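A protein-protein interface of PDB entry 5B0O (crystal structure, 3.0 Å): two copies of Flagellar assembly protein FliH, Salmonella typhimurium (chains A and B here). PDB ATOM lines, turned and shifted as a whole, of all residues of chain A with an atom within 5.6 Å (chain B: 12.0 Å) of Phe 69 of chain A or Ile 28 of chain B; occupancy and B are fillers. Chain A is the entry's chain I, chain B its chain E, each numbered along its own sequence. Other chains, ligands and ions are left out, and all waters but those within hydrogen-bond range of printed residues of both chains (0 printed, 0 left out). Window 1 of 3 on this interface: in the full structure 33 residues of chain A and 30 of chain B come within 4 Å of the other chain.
Among the printed residues, pairs that only touch across the chains: Phe 69 of chain A with Leu 32 of chain B (3.4 Å), Leu 63 of chain A with Met 35 of chain B (3.5 Å), Glu 66 of chain A with Met 35 of chain B (3.5 Å), Leu 68 of chain A with Ile 28 of chain B (3.7 Å), Phe 69 of chain A with Met 35 of chain B (3.7 Å), Phe 17 of chain A with Ile 28 of chain B (3.8 Å), Phe 17 of chain A with Leu 21 of chain B (3.9 Å) and Phe 69 of chain A with Ile 28 of chain B (3.9 Å).
Phe 17 of chain A touches Leu 21 of chain B, but with the chains exchanged Leu 21 of chain A does not touch Phe 17 of chain B (10.3 Å).
Positions printed for both chains: 17, 21, 24 and 25.
The side-chain carboxylate (OE2) of Glu 66 of chain A lies close to the backbone NH (N) of Leu 68 of chain A, at 3.3 Å.
O of Glu 66 of chain A is in hydrogen-bond range of OG of Ser 70 of chain A (3.5 Å).
Printed residues of chain B within 4 Å of Phe 17 of chain A: Leu 21 (3.9 Å) and Ile 28 (3.8 Å).
No residue of chain B comes within 4 Å of Leu 21 of chain A.
Asp 25 of chain A touches none of the printed residues of chain B.
Phe 69 of chain A touches just these residues of chain B: Ile 28 (3.9 Å), Leu 32 (3.4 Å) and Met 35 (3.7 Å).
No residue of chain B comes within 4 Å of Ser 70 of chain A.
Gly 71 of chain A touches none of the printed residues of chain B.
Of the printed residues of chain A, Leu 21 of chain B touches Phe 17.
Asp 22 of chain B touches none of the printed residues of chain A.
Of chain A, only Phe 17 (3.8 Å), Leu 68 (3.7 Å) and Phe 69 (3.9 Å) come within 4 Å of Ile 28 of chain B.
Of the printed residues of chain A, Arg 31 of chain B touches Glu 66 (2.9 Å).
Printed residues of chain A within 4 Å of Leu 32 of chain B: Phe 69 (3.4 Å).
Of the printed residues of chain A, Met 35 of chain B touches Leu 63, Glu 66 and Phe 69.
The nearest residue of chain A that does not touch Ile 28 of chain B is Leu 21 of chain A (4.7 Å).
The nearest printed residue of chain A that does not touch Arg 31 of chain B is Phe 69 of chain A (4.8 Å).
Along chain B the printed residues that touch a printed residue of chain A span positions 21 to 35.
Among the printed residues, 9 pairs touch across the chains.
Among the printed residues, Asp or Glu carboxylates within 4 Å of a Lys or Arg side-chain nitrogen of the other chain: Glu 66 of chain A with Arg 31 of chain B (2.9 Å).
The side-chain carboxylate (OE1) of Glu 66 of chain A lies within salt-bridge range of the guanidinium group (NE) of Arg 31 of chain B (2.9 Å).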
ATOM      1  N   PHE A  17      -7.832   8.805   2.801  1.00  0.00           N
ATOM      2  CA  PHE A  17      -7.369   7.889   1.766  1.00  0.00           C
ATOM      3  C   PHE A  17      -7.847   6.466   2.021  1.00  0.00           C
ATOM      4  O   PHE A  17      -8.637   5.930   1.252  1.00  0.00           O
ATOM      5  CB  PHE A  17      -5.847   7.912   1.644  1.00  0.00           C
ATOM      6  CG  PHE A  17      -5.320   7.096   0.495  1.00  0.00           C
ATOM      7  CD1 PHE A  17      -4.493   6.008   0.721  1.00  0.00           C
ATOM      8  CD2 PHE A  17      -5.663   7.414  -0.811  1.00  0.00           C
ATOM      9  CE1 PHE A  17      -4.013   5.255  -0.342  1.00  0.00           C
ATOM     10  CE2 PHE A  17      -5.188   6.666  -1.869  1.00  0.00           C
ATOM     11  CZ  PHE A  17      -4.364   5.586  -1.634  1.00  0.00           C
ATOM     12  N   LEU A  21     -10.415   3.972  -0.123  1.00  0.00           N
ATOM     13  CA  LEU A  21     -10.100   2.615  -0.571  1.00  0.00           C
ATOM     14  C   LEU A  21     -11.134   1.599  -0.068  1.00  0.00           C
ATOM     15  O   LEU A  21     -11.546   0.706  -0.805  1.00  0.00           O
ATOM     16  CB  LEU A  21      -8.688   2.204  -0.130  1.00  0.00           C
ATOM     17  CG  LEU A  21      -7.488   2.744  -0.915  1.00  0.00           C
ATOM     18  CD1 LEU A  21      -6.174   2.297  -0.289  1.00  0.00           C
ATOM     19  CD2 LEU A  21      -7.552   2.304  -2.363  1.00  0.00           C
ATOM     20  N   LEU A  24     -14.567   1.608  -1.819  1.00  0.00           N
ATOM     21  CA  LEU A  24     -14.516   0.914  -3.101  1.00  0.00           C
ATOM     22  C   LEU A  24     -15.259  -0.414  -3.062  1.00  0.00           C
ATOM     23  O   LEU A  24     -16.060  -0.711  -3.945  1.00  0.00           O
ATOM     24  CB  LEU A  24     -13.074   0.666  -3.545  1.00  0.00           C
ATOM     25  CG  LEU A  24     -12.295   1.785  -4.231  1.00  0.00           C
ATOM     26  CD1 LEU A  24     -11.043   1.205  -4.853  1.00  0.00           C
ATOM     27  CD2 LEU A  24     -13.130   2.486  -5.283  1.00  0.00           C
ATOM     28  N   ASP A  25     -15.001  -1.210  -2.033  1.00  0.00           N
ATOM     29  CA  ASP A  25     -15.495  -2.581  -2.027  1.00  0.00           C
ATOM     30  C   ASP A  25     -17.017  -2.661  -2.145  1.00  0.00           C
ATOM     31  O   ASP A  25     -17.539  -3.457  -2.921  1.00  0.00           O
ATOM     32  CB  ASP A  25     -14.958  -3.355  -0.817  1.00  0.00           C
ATOM     33  CG  ASP A  25     -13.458  -3.612  -0.915  1.00  0.00           C
ATOM     34  OD1 ASP A  25     -12.954  -3.747  -2.052  1.00  0.00           O
ATOM     35  OD2 ASP A  25     -12.781  -3.676   0.135  1.00  0.00           O
ATOM     36  N   LEU A  63     -10.764  -7.335  -8.541  1.00  0.00           N
ATOM     37  CA  LEU A  63     -10.510  -6.401  -7.462  1.00  0.00           C
ATOM     38  C   LEU A  63      -9.649  -7.022  -6.378  1.00  0.00           C
ATOM     39  O   LEU A  63      -8.725  -6.390  -5.866  1.00  0.00           O
ATOM     40  CB  LEU A  63     -11.836  -5.957  -6.858  1.00  0.00           C
ATOM     41  CG  LEU A  63     -12.576  -4.937  -7.709  1.00  0.00           C
ATOM     42  CD1 LEU A  63     -14.084  -5.039  -7.535  1.00  0.00           C
ATOM     43  CD2 LEU A  63     -12.069  -3.546  -7.369  1.00  0.00           C
ATOM     44  N   GLU A  66      -5.843  -6.801  -6.722  1.00  0.00           N
ATOM     45  CA  GLU A  66      -5.048  -5.605  -6.480  1.00  0.00           C
ATOM     46  C   GLU A  66      -4.804  -5.453  -4.987  1.00  0.00           C
ATOM     47  O   GLU A  66      -5.721  -5.148  -4.226  1.00  0.00           O
ATOM     48  CB  GLU A  66      -5.738  -4.358  -7.045  1.00  0.00           C
ATOM     49  CG  GLU A  66      -4.990  -3.057  -6.793  1.00  0.00           C
ATOM     50  CD  GLU A  66      -3.539  -3.115  -7.234  1.00  0.00           C
ATOM     51  OE1 GLU A  66      -3.277  -3.083  -8.454  1.00  0.00           O
ATOM     52  OE2 GLU A  66      -2.653  -3.181  -6.359  1.00  0.00           O
ATOM     53  N   PRO A  67      -3.558  -5.681  -4.563  1.00  0.00           N
ATOM     54  CA  PRO A  67      -3.161  -5.622  -3.157  1.00  0.00           C
ATOM     55  C   PRO A  67      -3.598  -4.321  -2.495  1.00  0.00           C
ATOM     56  O   PRO A  67      -3.943  -4.339  -1.319  1.00  0.00           O
ATOM     57  CB  PRO A  67      -1.635  -5.687  -3.226  1.00  0.00           C
ATOM     58  CG  PRO A  67      -1.361  -6.426  -4.470  1.00  0.00           C
ATOM     59  CD  PRO A  67      -2.429  -6.023  -5.440  1.00  0.00           C
ATOM     60  N   LEU A  68      -3.586  -3.217  -3.233  1.00  0.00           N
ATOM     61  CA  LEU A  68      -3.949  -1.930  -2.654  1.00  0.00           C
ATOM     62  C   LEU A  68      -5.382  -1.963  -2.136  1.00  0.00           C
ATOM     63  O   LEU A  68      -5.687  -1.407  -1.081  1.00  0.00           O
ATOM     64  CB  LEU A  68      -3.769  -0.803  -3.673  1.00  0.00           C
ATOM     65  CG  LEU A  68      -3.878   0.624  -3.136  1.00  0.00           C
ATOM     66  CD1 LEU A  68      -2.955   0.813  -1.947  1.00  0.00           C
ATOM     67  CD2 LEU A  68      -3.554   1.626  -4.227  1.00  0.00           C
ATOM     68  N   PHE A  69      -6.258  -2.612  -2.894  1.00  0.00           N
ATOM     69  CA  PHE A  69      -7.644  -2.799  -2.489  1.00  0.00           C
ATOM     70  C   PHE A  69      -7.821  -3.985  -1.527  1.00  0.00           C
ATOM     71  O   PHE A  69      -8.583  -3.903  -0.557  1.00  0.00           O
ATOM     72  CB  PHE A  69      -8.535  -2.971  -3.723  1.00  0.00           C
ATOM     73  CG  PHE A  69      -8.377  -1.880  -4.746  1.00  0.00           C
ATOM     74  CD1 PHE A  69      -8.723  -2.103  -6.069  1.00  0.00           C
ATOM     75  CD2 PHE A  69      -7.885  -0.632  -4.390  1.00  0.00           C
ATOM     76  CE1 PHE A  69      -8.580  -1.108  -7.018  1.00  0.00           C
ATOM     77  CE2 PHE A  69      -7.742   0.371  -5.337  1.00  0.00           C
ATOM     78  CZ  PHE A  69      -8.092   0.129  -6.652  1.00  0.00           C
ATOM     79  N   SER A  70      -7.117  -5.082  -1.806  1.00  0.00           N
ATOM     80  CA  SER A  70      -7.250  -6.302  -1.009  1.00  0.00           C
ATOM     81  C   SER A  70      -6.471  -6.226   0.300  1.00  0.00           C
ATOM     82  O   SER A  70      -6.951  -6.662   1.346  1.00  0.00           O
ATOM     83  CB  SER A  70      -6.809  -7.531  -1.808  1.00  0.00           C
ATOM     84  OG  SER A  70      -5.399  -7.644  -1.856  1.00  0.00           O
ATOM     85  N   GLY A  71      -5.266  -5.672   0.228  1.00  0.00           N
ATOM     86  CA  GLY A  71      -4.427  -5.477   1.396  1.00  0.00           C
ATOM     87  C   GLY A  71      -4.475  -4.052   1.912  1.00  0.00           C
ATOM     88  O   GLY A  71      -5.510  -3.384   1.847  1.00  0.00           O
ATOM     89  N   PHE B  17       3.717  13.950   1.479  1.00  0.00           N
ATOM     90  CA  PHE B  17       2.755  12.871   1.658  1.00  0.00           C
ATOM     91  C   PHE B  17       1.433  13.195   0.957  1.00  0.00           C
ATOM     92  O   PHE B  17       0.776  12.311   0.407  1.00  0.00           O
ATOM     93  CB  PHE B  17       2.539  12.626   3.154  1.00  0.00           C
ATOM     94  CG  PHE B  17       1.572  11.521   3.464  1.00  0.00           C
ATOM     95  CD1 PHE B  17       1.873  10.207   3.150  1.00  0.00           C
ATOM     96  CD2 PHE B  17       0.375  11.795   4.100  1.00  0.00           C
ATOM     97  CE1 PHE B  17       0.982   9.190   3.445  1.00  0.00           C
ATOM     98  CE2 PHE B  17      -0.513  10.784   4.399  1.00  0.00           C
ATOM     99  CZ  PHE B  17      -0.210   9.481   4.072  1.00  0.00           C
ATOM    100  N   GLN B  18       1.051  14.469   0.980  1.00  0.00           N
ATOM    101  CA  GLN B  18      -0.147  14.925   0.288  1.00  0.00           C
ATOM    102  C   GLN B  18       0.006  14.752  -1.211  1.00  0.00           C
ATOM    103  O   GLN B  18      -0.879  14.225  -1.880  1.00  0.00           O
ATOM    104  CB  GLN B  18      -0.408  16.399   0.586  1.00  0.00           C
ATOM    105  CG  GLN B  18      -1.580  16.992  -0.182  1.00  0.00           C
ATOM    106  CD  GLN B  18      -2.916  16.641   0.439  1.00  0.00           C
ATOM    107  OE1 GLN B  18      -3.182  16.976   1.594  1.00  0.00           O
ATOM    108  NE2 GLN B  18      -3.764  15.960  -0.324  1.00  0.00           N
ATOM    109  N   ASN B  19       1.134  15.210  -1.737  1.00  0.00           N
ATOM    110  CA  ASN B  19       1.402  15.102  -3.164  1.00  0.00           C
ATOM    111  C   ASN B  19       1.404  13.657  -3.642  1.00  0.00           C
ATOM    112  O   ASN B  19       0.854  13.342  -4.695  1.00  0.00           O
ATOM    113  CB  ASN B  19       2.729  15.774  -3.521  1.00  0.00           C
ATOM    114  CG  ASN B  19       2.578  17.255  -3.781  1.00  0.00           C
ATOM    115  OD1 ASN B  19       1.622  17.886  -3.327  1.00  0.00           O
ATOM    116  ND2 ASN B  19       3.521  17.820  -4.526  1.00  0.00           N
ATOM    117  N   THR B  20       2.021  12.776  -2.865  1.00  0.00           N
ATOM    118  CA  THR B  20       2.118  11.376  -3.255  1.00  0.00           C
ATOM    119  C   THR B  20       0.745  10.731  -3.448  1.00  0.00           C
ATOM    120  O   THR B  20       0.537   9.981  -4.396  1.00  0.00           O
ATOM    121  CB  THR B  20       2.959  10.560  -2.257  1.00  0.00           C
ATOM    122  OG1 THR B  20       4.329  10.975  -2.335  1.00  0.00           O
ATOM    123  CG2 THR B  20       2.869   9.075  -2.572  1.00  0.00           C
ATOM    124  N   LEU B  21      -0.193  11.027  -2.555  1.00  0.00           N
ATOM    125  CA  LEU B  21      -1.535  10.470  -2.670  1.00  0.00           C
ATOM    126  C   LEU B  21      -2.234  11.012  -3.908  1.00  0.00           C
ATOM    127  O   LEU B  21      -2.816  10.255  -4.682  1.00  0.00           O
ATOM    128  CB  LEU B  21      -2.359  10.761  -1.418  1.00  0.00           C
ATOM    129  CG  LEU B  21      -1.832  10.160  -0.115  1.00  0.00           C
ATOM    130  CD1 LEU B  21      -2.854  10.333   0.995  1.00  0.00           C
ATOM    131  CD2 LEU B  21      -1.486   8.690  -0.295  1.00  0.00           C
ATOM    132  N   ASP B  22      -2.170  12.327  -4.091  1.00  0.00           N
ATOM    133  CA  ASP B  22      -2.751  12.968  -5.263  1.00  0.00           C
ATOM    134  C   ASP B  22      -2.211  12.338  -6.540  1.00  0.00           C
ATOM    135  O   ASP B  22      -2.917  12.216  -7.536  1.00  0.00           O
ATOM    136  CB  ASP B  22      -2.458  14.469  -5.236  1.00  0.00           C
ATOM    137  CG  ASP B  22      -3.115  15.169  -4.055  1.00  0.00           C
ATOM    138  OD1 ASP B  22      -3.574  14.461  -3.129  1.00  0.00           O
ATOM    139  OD2 ASP B  22      -3.169  16.421  -4.055  1.00  0.00           O
ATOM    140  N   ALA B  23      -0.956  11.915  -6.492  1.00  0.00           N
ATOM    141  CA  ALA B  23      -0.317  11.280  -7.634  1.00  0.00           C
ATOM    142  C   ALA B  23      -1.014   9.984  -8.018  1.00  0.00           C
ATOM    143  O   ALA B  23      -1.068   9.630  -9.192  1.00  0.00           O
ATOM    144  CB  ALA B  23       1.148  11.016  -7.337  1.00  0.00           C
ATOM    145  N   LEU B  24      -1.532   9.273  -7.024  1.00  0.00           N
ATOM    146  CA  LEU B  24      -2.166   7.979  -7.260  1.00  0.00           C
ATOM    147  C   LEU B  24      -3.587   8.098  -7.802  1.00  0.00           C
ATOM    148  O   LEU B  24      -4.104   7.149  -8.386  1.00  0.00           O
ATOM    149  CB  LEU B  24      -2.160   7.136  -5.984  1.00  0.00           C
ATOM    150  CG  LEU B  24      -0.776   6.665  -5.544  1.00  0.00           C
ATOM    151  CD1 LEU B  24      -0.789   6.243  -4.089  1.00  0.00           C
ATOM    152  CD2 LEU B  24      -0.284   5.539  -6.437  1.00  0.00           C
ATOM    153  N   ASP B  25      -4.214   9.255  -7.624  1.00  0.00           N
ATOM    154  CA  ASP B  25      -5.610   9.397  -8.013  1.00  0.00           C
ATOM    155  C   ASP B  25      -5.854   9.001  -9.460  1.00  0.00           C
ATOM    156  O   ASP B  25      -6.841   8.346  -9.761  1.00  0.00           O
ATOM    157  CB  ASP B  25      -6.112  10.811  -7.752  1.00  0.00           C
ATOM    158  CG  ASP B  25      -6.075  11.169  -6.289  1.00  0.00           C
ATOM    159  OD1 ASP B  25      -5.969  10.237  -5.464  1.00  0.00           O
ATOM    160  OD2 ASP B  25      -6.163  12.373  -5.968  1.00  0.00           O
ATOM    161  N   SER B  26      -4.954   9.396 -10.352  1.00  0.00           N
ATOM    162  CA  SER B  26      -5.063   9.035 -11.764  1.00  0.00           C
ATOM    163  C   SER B  26      -4.603   7.604 -12.023  1.00  0.00           C
ATOM    164  O   SER B  26      -5.104   6.934 -12.930  1.00  0.00           O
ATOM    165  CB  SER B  26      -4.247  10.001 -12.615  1.00  0.00           C
ATOM    166  OG  SER B  26      -3.018  10.323 -11.981  1.00  0.00           O
ATOM    167  N   VAL B  27      -3.642   7.145 -11.228  1.00  0.00           N
ATOM    168  CA  VAL B  27      -3.119   5.798 -11.365  1.00  0.00           C
ATOM    169  C   VAL B  27      -4.159   4.797 -10.869  1.00  0.00           C
ATOM    170  O   VAL B  27      -4.434   3.795 -11.525  1.00  0.00           O
ATOM    171  CB  VAL B  27      -1.807   5.646 -10.575  1.00  0.00           C
ATOM    172  CG1 VAL B  27      -1.162   4.286 -10.824  1.00  0.00           C
ATOM    173  CG2 VAL B  27      -0.843   6.773 -10.938  1.00  0.00           C
ATOM    174  N   ILE B  28      -4.742   5.091  -9.714  1.00  0.00           N
ATOM    175  CA  ILE B  28      -5.748   4.233  -9.100  1.00  0.00           C
ATOM    176  C   ILE B  28      -7.045   4.167  -9.899  1.00  0.00           C
ATOM    177  O   ILE B  28      -7.635   3.100 -10.054  1.00  0.00           O
ATOM    178  CB  ILE B  28      -6.042   4.685  -7.662  1.00  0.00           C
ATOM    179  CG1 ILE B  28      -4.814   4.433  -6.786  1.00  0.00           C
ATOM    180  CG2 ILE B  28      -7.254   3.961  -7.108  1.00  0.00           C
ATOM    181  CD1 ILE B  28      -4.974   4.896  -5.362  1.00  0.00           C
ATOM    182  N   ALA B  29      -7.496   5.310 -10.397  1.00  0.00           N
ATOM    183  CA  ALA B  29      -8.668   5.335 -11.260  1.00  0.00           C
ATOM    184  C   ALA B  29      -8.403   4.493 -12.493  1.00  0.00           C
ATOM    185  O   ALA B  29      -9.235   3.702 -12.914  1.00  0.00           O
ATOM    186  CB  ALA B  29      -9.006   6.756 -11.656  1.00  0.00           C
ATOM    187  N   SER B  30      -7.229   4.684 -13.077  1.00  0.00           N
ATOM    188  CA  SER B  30      -6.840   3.953 -14.272  1.00  0.00           C
ATOM    189  C   SER B  30      -6.815   2.456 -14.005  1.00  0.00           C
ATOM    190  O   SER B  30      -7.407   1.670 -14.740  1.00  0.00           O
ATOM    191  CB  SER B  30      -5.479   4.438 -14.760  1.00  0.00           C
ATOM    192  OG  SER B  30      -4.978   3.597 -15.782  1.00  0.00           O
ATOM    193  N   ARG B  31      -6.141   2.069 -12.932  1.00  0.00           N
ATOM    194  CA  ARG B  31      -6.144   0.685 -12.487  1.00  0.00           C
ATOM    195  C   ARG B  31      -7.570   0.118 -12.433  1.00  0.00           C
ATOM    196  O   ARG B  31      -7.799  -1.047 -12.764  1.00  0.00           O
ATOM    197  CB  ARG B  31      -5.506   0.589 -11.108  1.00  0.00           C
ATOM    198  CG  ARG B  31      -5.380  -0.821 -10.585  1.00  0.00           C
ATOM    199  CD  ARG B  31      -4.539  -1.644 -11.538  1.00  0.00           C
ATOM    200  NE  ARG B  31      -4.406  -3.028 -11.102  1.00  0.00           N
ATOM    201  CZ  ARG B  31      -5.260  -3.993 -11.421  1.00  0.00           C
ATOM    202  NH1 ARG B  31      -6.322  -3.731 -12.172  1.00  0.00           N
ATOM    203  NH2 ARG B  31      -5.054  -5.224 -10.983  1.00  0.00           N
ATOM    204  N   LEU B  32      -8.528   0.934 -12.004  1.00  0.00           N
ATOM    205  CA  LEU B  32      -9.906   0.470 -11.886  1.00  0.00           C
ATOM    206  C   LEU B  32     -10.543   0.261 -13.262  1.00  0.00           C
ATOM    207  O   LEU B  32     -11.280  -0.701 -13.468  1.00  0.00           O
ATOM    208  CB  LEU B  32     -10.732   1.422 -11.009  1.00  0.00           C
ATOM    209  CG  LEU B  32     -10.497   1.360  -9.493  1.00  0.00           C
ATOM    210  CD1 LEU B  32     -11.051   2.587  -8.772  1.00  0.00           C
ATOM    211  CD2 LEU B  32     -11.086   0.083  -8.922  1.00  0.00           C
ATOM    212  N   MET B  33     -10.253   1.165 -14.194  1.00  0.00           N
ATOM    213  CA  MET B  33     -10.640   0.999 -15.591  1.00  0.00           C
ATOM    214  C   MET B  33     -10.105  -0.304 -16.168  1.00  0.00           C
ATOM    215  O   MET B  33     -10.802  -0.992 -16.908  1.00  0.00           O
ATOM    216  CB  MET B  33     -10.080   2.140 -16.426  1.00  0.00           C
ATOM    217  CG  MET B  33     -10.409   3.509 -15.901  1.00  0.00           C
ATOM    218  SD  MET B  33      -9.802   4.762 -17.024  1.00  0.00           S
ATOM    219  CE  MET B  33     -10.338   6.231 -16.157  1.00  0.00           C
ATOM    220  N   GLN B  34      -8.853  -0.623 -15.852  1.00  0.00           N
ATOM    221  CA  GLN B  34      -8.233  -1.827 -16.380  1.00  0.00           C
ATOM    222  C   GLN B  34      -9.043  -3.040 -15.973  1.00  0.00           C
ATOM    223  O   GLN B  34      -9.175  -3.983 -16.747  1.00  0.00           O
ATOM    224  CB  GLN B  34      -6.783  -1.975 -15.902  1.00  0.00           C
ATOM    225  CG  GLN B  34      -5.766  -1.144 -16.679  1.00  0.00           C
ATOM    226  CD  GLN B  34      -4.346  -1.317 -16.162  1.00  0.00           C
ATOM    227  OE1 GLN B  34      -4.135  -1.797 -15.046  1.00  0.00           O
ATOM    228  NE2 GLN B  34      -3.367  -0.928 -16.971  1.00  0.00           N
ATOM    229  N   MET B  35      -9.585  -3.012 -14.759  1.00  0.00           N
ATOM    230  CA  MET B  35     -10.358  -4.140 -14.255  1.00  0.00           C
ATOM    231  C   MET B  35     -11.612  -4.317 -15.086  1.00  0.00           C
ATOM    232  O   MET B  35     -11.878  -5.407 -15.574  1.00  0.00           O
ATOM    233  CB  MET B  35     -10.706  -3.957 -12.779  1.00  0.00           C
ATOM    234  CG  MET B  35      -9.496  -3.920 -11.855  1.00  0.00           C
ATOM    235  SD  MET B  35      -9.950  -3.901 -10.111  1.00  0.00           S
ATOM    236  CE  MET B  35      -8.334  -4.027  -9.358  1.00  0.00           C
ATOM    237  N   ALA B  36     -12.368  -3.241 -15.272  1.00  0.00           N
ATOM    238  CA  ALA B  36     -13.561  -3.292 -16.115  1.00  0.00           C
ATOM    239  C   ALA B  36     -13.231  -3.682 -17.555  1.00  0.00           C
ATOM    240  O   ALA B  36     -14.004  -4.377 -18.202  1.00  0.00           O
ATOM    241  CB  ALA B  36     -14.303  -1.967 -16.079  1.00  0.00           C
ATOM    242  N   LEU B  37     -12.090  -3.226 -18.062  1.00  0.00           N
ATOM    243  CA  LEU B  37     -11.694  -3.544 -19.431  1.00  0.00           C
ATOM    244  C   LEU B  37     -11.420  -5.033 -19.610  1.00  0.00           C
ATOM    245  O   LEU B  37     -11.869  -5.640 -20.581  1.00  0.00           O
ATOM    246  CB  LEU B  37     -10.486  -2.714 -19.862  1.00  0.00           C
ATOM    247  CG  LEU B  37     -10.813  -1.281 -20.268  1.00  0.00           C
ATOM    248  CD1 LEU B  37      -9.566  -0.548 -20.729  1.00  0.00           C
ATOM    249  CD2 LEU B  37     -11.860  -1.269 -21.359  1.00  0.00           C
ATOM    250  N   ALA B 135      -8.252   5.068 -23.115  1.00  0.00           N
ATOM    251  CA  ALA B 135      -8.042   4.890 -21.684  1.00  0.00           C
ATOM    252  C   ALA B 135      -6.603   5.162 -21.247  1.00  0.00           C
ATOM    253  O   ALA B 135      -6.361   5.612 -20.132  1.00  0.00           O
ATOM    254  CB  ALA B 135      -8.480   3.491 -21.263  1.00  0.00           C
ATOM    255  N   ALA B 136      -5.650   4.860 -22.118  1.00  0.00           N
ATOM    256  CA  ALA B 136      -4.243   5.106 -21.822  1.00  0.00           C
ATOM    257  C   ALA B 136      -3.515   5.773 -22.983  1.00  0.00           C
ATOM    258  O   ALA B 136      -2.916   5.101 -23.819  1.00  0.00           O
ATOM    259  CB  ALA B 136      -3.545   3.820 -21.440  1.00  0.00           C
